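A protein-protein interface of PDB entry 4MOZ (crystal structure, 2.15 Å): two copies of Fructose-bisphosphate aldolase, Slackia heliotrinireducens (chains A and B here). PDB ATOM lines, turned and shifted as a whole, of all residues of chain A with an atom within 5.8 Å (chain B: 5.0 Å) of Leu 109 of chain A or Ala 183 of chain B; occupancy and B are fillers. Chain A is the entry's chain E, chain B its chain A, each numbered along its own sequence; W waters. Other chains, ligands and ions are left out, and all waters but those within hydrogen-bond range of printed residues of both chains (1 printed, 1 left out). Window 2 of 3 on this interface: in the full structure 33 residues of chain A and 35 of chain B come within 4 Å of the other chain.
Water W1 lies within hydrogen-bond range of the backbone carbonyl oxygen of Leu 109 of chain A (2.7 Å) and the backbone carbonyl oxygen of Ala 183 of chain B (3.0 Å).
Of the 9 printed residues of chain B, 5 touch a printed residue of chain A. Hydrophobic or aromatic side chains of chain B within 4 Å of the printed part of chain A: Ala 183. Of the 8 printed residues of chain A, 4 touch a printed residue of chain B. Hydrophobic or aromatic side chains of chain A within 4 Å of the printed part of chain B: Leu 109 and Val 110. Among the printed residues, no Asp or Glu carboxylate lies within 4 Å of a Lys or Arg side-chain nitrogen of the other chain.
Of the printed residues of chain B, Thr 107 of chain A touches Glu 152. Asn 108 of chain A touches none of the printed residues of chain B. Leu 109 of chain A touches just these residues of chain B: Leu 147, Gly 148 and Ala 183. Of the printed residues of chain B, Val 110 of chain A touches Gly 148 (3.4 Å) and Ala 183 (3.9 Å). Of the printed residues of chain A, Gly 148 of chain B touches Leu 109 and Val 110. Of the printed residues of chain A, Glu 152 of chain B touches Thr 107 (2.8 Å). Of the printed residues of chain A, Lys 182 of chain B touches Gln 114. Of chain A, only Leu 109, Val 110 and Gln 114 come within 4 Å of Ala 183 of chain B. Gly 185 of chain B touches none of the printed residues of chain A. The nearest printed residue of chain B that does not touch Val 110 of chain A is Glu 152 of chain B (5.8 Å).
The side-chain hydroxyl of Thr 107 of chain A sits close to the backbone NH of Leu 109 of chain A (3.4 Å). The backbone NH (N) of Gly 148 of chain B is in hydrogen-bond range of the side-chain carboxylate (OE1) of Glu 152 of chain B (2.8 Å).
OE1 of Glu 152 of chain B sits at hydrogen-bond distance from OG1 of Thr 107 of chain A, at 2.8 Å.
Among the printed residues, merely in contact across the chains: Gln 114 of chain A with Ala 183 of chain B (3.3 Å), Val 110 of chain A with Gly 148 of chain B (3.4 Å), Leu 109 of chain A with Ala 183 of chain B (3.4 Å), Gln 114 of chain A with Lys 182 of chain B (3.6 Å), Leu 109 of chain A with Gly 148 of chain B (3.7 Å), Leu 109 of chain A with Leu 147 of chain B (3.8 Å) and Val 110 of chain A with Ala 183 of chain B (3.9 Å).
No position is printed for both chains. Of the 8 pairs that touch across the chains among the printed residues, none has its exchanged pair printed and touching as well.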
ATOM      1  N   GLU A  47       7.960  14.208   6.344  1.00  0.00           N
ATOM      2  CA  GLU A  47       8.183  12.782   6.095  1.00  0.00           C
ATOM      3  C   GLU A  47       9.519  12.447   5.433  1.00  0.00           C
ATOM      4  O   GLU A  47      10.236  11.564   5.908  1.00  0.00           O
ATOM      5  CB  GLU A  47       7.018  12.180   5.301  1.00  0.00           C
ATOM      6  CG  GLU A  47       5.678  12.249   6.023  1.00  0.00           C
ATOM      7  CD  GLU A  47       5.637  11.432   7.305  1.00  0.00           C
ATOM      8  OE1 GLU A  47       6.200  10.315   7.325  1.00  0.00           O
ATOM      9  OE2 GLU A  47       5.029  11.904   8.296  1.00  0.00           O
ATOM     10  N   LEU A  49      11.744  15.018   4.515  1.00  0.00           N
ATOM     11  CA  LEU A  49      12.490  16.275   4.595  1.00  0.00           C
ATOM     12  C   LEU A  49      12.436  17.041   3.265  1.00  0.00           C
ATOM     13  O   LEU A  49      11.344  17.326   2.778  1.00  0.00           O
ATOM     14  CB  LEU A  49      13.922  16.047   5.112  1.00  0.00           C
ATOM     15  CG  LEU A  49      14.023  15.463   6.531  1.00  0.00           C
ATOM     16  CD1 LEU A  49      15.469  15.209   6.917  1.00  0.00           C
ATOM     17  CD2 LEU A  49      13.353  16.355   7.570  1.00  0.00           C
ATOM     18  N   THR A 107      10.085  12.421  10.654  1.00  0.00           N
ATOM     19  CA  THR A 107      11.095  12.437   9.595  1.00  0.00           C
ATOM     20  C   THR A 107      11.549  11.009   9.294  1.00  0.00           C
ATOM     21  O   THR A 107      11.237  10.082  10.041  1.00  0.00           O
ATOM     22  CB  THR A 107      12.320  13.301   9.955  1.00  0.00           C
ATOM     23  OG1 THR A 107      13.188  12.567  10.823  1.00  0.00           O
ATOM     24  CG2 THR A 107      11.897  14.608  10.628  1.00  0.00           C
ATOM     25  N   ASN A 108      12.290  10.840   8.203  1.00  0.00           N
ATOM     26  CA  ASN A 108      12.775   9.528   7.783  1.00  0.00           C
ATOM     27  C   ASN A 108      14.251   9.321   8.119  1.00  0.00           C
ATOM     28  O   ASN A 108      14.924   8.498   7.500  1.00  0.00           O
ATOM     29  CB  ASN A 108      12.542   9.330   6.274  1.00  0.00           C
ATOM     30  CG  ASN A 108      13.308  10.337   5.413  1.00  0.00           C
ATOM     31  OD1 ASN A 108      13.669  11.429   5.868  1.00  0.00           O
ATOM     32  ND2 ASN A 108      13.554   9.973   4.161  1.00  0.00           N
ATOM     33  N   LEU A 109      14.754  10.080   9.089  1.00  0.00           N
ATOM     34  CA  LEU A 109      16.157   9.963   9.495  1.00  0.00           C
ATOM     35  C   LEU A 109      16.437   8.665  10.253  1.00  0.00           C
ATOM     36  O   LEU A 109      17.458   8.020  10.020  1.00  0.00           O
ATOM     37  CB  LEU A 109      16.602  11.184  10.307  1.00  0.00           C
ATOM     38  CG  LEU A 109      16.681  12.498   9.522  1.00  0.00           C
ATOM     39  CD1 LEU A 109      16.664  13.699  10.451  1.00  0.00           C
ATOM     40  CD2 LEU A 109      17.907  12.518   8.618  1.00  0.00           C
ATOM     41  N   VAL A 110      15.533   8.284  11.154  1.00  0.00           N
ATOM     42  CA  VAL A 110      15.677   7.025  11.872  1.00  0.00           C
ATOM     43  C   VAL A 110      15.033   5.919  11.045  1.00  0.00           C
ATOM     44  O   VAL A 110      13.819   5.910  10.835  1.00  0.00           O
ATOM     45  CB  VAL A 110      15.081   7.086  13.301  1.00  0.00           C
ATOM     46  CG1 VAL A 110      15.162   5.723  13.984  1.00  0.00           C
ATOM     47  CG2 VAL A 110      15.802   8.134  14.135  1.00  0.00           C
ATOM     48  N   LYS A 111      15.860   5.001  10.560  1.00  0.00           N
ATOM     49  CA  LYS A 111      15.379   3.893   9.743  1.00  0.00           C
ATOM     50  C   LYS A 111      14.814   2.788  10.633  1.00  0.00           C
ATOM     51  O   LYS A 111      15.162   2.691  11.815  1.00  0.00           O
ATOM     52  CB  LYS A 111      16.501   3.351   8.838  1.00  0.00           C
ATOM     53  CG  LYS A 111      17.206   4.391   7.969  1.00  0.00           C
ATOM     54  CD  LYS A 111      16.248   5.100   7.018  1.00  0.00           C
ATOM     55  CE  LYS A 111      16.944   6.209   6.240  1.00  0.00           C
ATOM     56  NZ  LYS A 111      15.967   7.000   5.440  1.00  0.00           N
ATOM     57  N   GLN A 114      17.159   0.705  12.735  1.00  0.00           N
ATOM     58  CA  GLN A 114      17.609   1.348  13.972  1.00  0.00           C
ATOM     59  C   GLN A 114      16.541   1.259  15.071  1.00  0.00           C
ATOM     60  O   GLN A 114      16.826   0.827  16.191  1.00  0.00           O
ATOM     61  CB  GLN A 114      18.003   2.810  13.733  1.00  0.00           C
ATOM     62  CG  GLN A 114      18.412   3.544  15.008  1.00  0.00           C
ATOM     63  CD  GLN A 114      18.612   5.039  14.817  1.00  0.00           C
ATOM     64  OE1 GLN A 114      18.693   5.527  13.695  1.00  0.00           O
ATOM     65  NE2 GLN A 114      18.695   5.774  15.923  1.00  0.00           N
ATOM     66  N   LEU B 147      15.901  16.768  15.281  1.00  0.00           N
ATOM     67  CA  LEU B 147      15.373  15.814  14.305  1.00  0.00           C
ATOM     68  C   LEU B 147      16.344  14.653  14.162  1.00  0.00           C
ATOM     69  O   LEU B 147      17.559  14.841  14.222  1.00  0.00           O
ATOM     70  CB  LEU B 147      15.152  16.482  12.944  1.00  0.00           C
ATOM     71  CG  LEU B 147      14.239  17.708  12.846  1.00  0.00           C
ATOM     72  CD1 LEU B 147      14.117  18.133  11.389  1.00  0.00           C
ATOM     73  CD2 LEU B 147      12.862  17.468  13.464  1.00  0.00           C
ATOM     74  N   GLY B 148      15.808  13.452  13.991  1.00  0.00           N
ATOM     75  CA  GLY B 148      16.649  12.271  13.821  1.00  0.00           C
ATOM     76  C   GLY B 148      17.169  11.680  15.114  1.00  0.00           C
ATOM     77  O   GLY B 148      17.856  10.661  15.096  1.00  0.00           O
ATOM     78  N   GLU B 152      13.016  12.295  18.949  1.00  0.00           N
ATOM     79  CA  GLU B 152      12.405  13.256  18.028  1.00  0.00           C
ATOM     80  C   GLU B 152      10.904  13.448  18.287  1.00  0.00           C
ATOM     81  O   GLU B 152      10.434  14.582  18.417  1.00  0.00           O
ATOM     82  CB  GLU B 152      12.641  12.822  16.573  1.00  0.00           C
ATOM     83  CG  GLU B 152      11.829  13.585  15.529  1.00  0.00           C
ATOM     84  CD  GLU B 152      11.970  13.005  14.125  1.00  0.00           C
ATOM     85  OE1 GLU B 152      13.052  13.186  13.517  1.00  0.00           O
ATOM     86  OE2 GLU B 152      10.997  12.382  13.622  1.00  0.00           O
ATOM     87  N   PRO B 179      19.238  18.824  13.578  1.00  0.00           N
ATOM     88  CA  PRO B 179      19.218  17.368  13.483  1.00  0.00           C
ATOM     89  C   PRO B 179      20.459  16.763  14.147  1.00  0.00           C
ATOM     90  O   PRO B 179      21.591  17.070  13.765  1.00  0.00           O
ATOM     91  CB  PRO B 179      19.185  17.119  11.978  1.00  0.00           C
ATOM     92  CG  PRO B 179      18.469  18.320  11.446  1.00  0.00           C
ATOM     93  CD  PRO B 179      18.980  19.465  12.278  1.00  0.00           C
ATOM     94  N   GLY B 181      21.869  13.075  16.397  1.00  0.00           N
ATOM     95  CA  GLY B 181      21.657  11.720  16.862  1.00  0.00           C
ATOM     96  C   GLY B 181      22.489  10.699  16.119  1.00  0.00           C
ATOM     97  O   GLY B 181      23.124  11.005  15.112  1.00  0.00           O
ATOM     98  N   LYS B 182      22.503   9.493  16.677  1.00  0.00           N
ATOM     99  CA  LYS B 182      22.956   8.261  16.040  1.00  0.00           C
ATOM    100  C   LYS B 182      22.701   8.253  14.526  1.00  0.00           C
ATOM    101  O   LYS B 182      23.606   7.992  13.729  1.00  0.00           O
ATOM    102  CB  LYS B 182      22.134   7.136  16.668  1.00  0.00           C
ATOM    103  CG  LYS B 182      22.813   5.820  16.942  1.00  0.00           C
ATOM    104  CD  LYS B 182      21.747   4.916  17.530  1.00  0.00           C
ATOM    105  CE  LYS B 182      22.332   3.794  18.354  1.00  0.00           C
ATOM    106  NZ  LYS B 182      21.276   3.190  19.207  1.00  0.00           N
ATOM    107  N   ALA B 183      21.455   8.544  14.152  1.00  0.00           N
ATOM    108  CA  ALA B 183      20.981   8.475  12.768  1.00  0.00           C
ATOM    109  C   ALA B 183      21.566   9.559  11.863  1.00  0.00           C
ATOM    110  O   ALA B 183      21.636   9.378  10.648  1.00  0.00           O
ATOM    111  CB  ALA B 183      19.458   8.546  12.740  1.00  0.00           C
ATOM    112  N   VAL B 184      21.976  10.676  12.460  1.00  0.00           N
ATOM    113  CA  VAL B 184      22.444  11.850  11.714  1.00  0.00           C
ATOM    114  C   VAL B 184      23.964  11.834  11.536  1.00  0.00           C
ATOM    115  O   VAL B 184      24.458  11.737  10.416  1.00  0.00           O
ATOM    116  CB  VAL B 184      21.988  13.169  12.390  1.00  0.00           C
ATOM    117  CG1 VAL B 184      22.431  14.375  11.581  1.00  0.00           C
ATOM    118  CG2 VAL B 184      20.474  13.187  12.561  1.00  0.00           C
ATOM    119  N   GLY B 185      24.697  11.938  12.642  1.00  0.00           N
ATOM    120  CA  GLY B 185      26.161  11.866  12.627  1.00  0.00           C
ATOM    121  C   GLY B 185      26.838  12.859  11.702  1.00  0.00           C
ATOM    122  O   GLY B 185      26.709  14.071  11.879  1.00  0.00           O
HETATM  123  O   HOH W   1      19.968   7.273   9.262  1.00  0.00           O
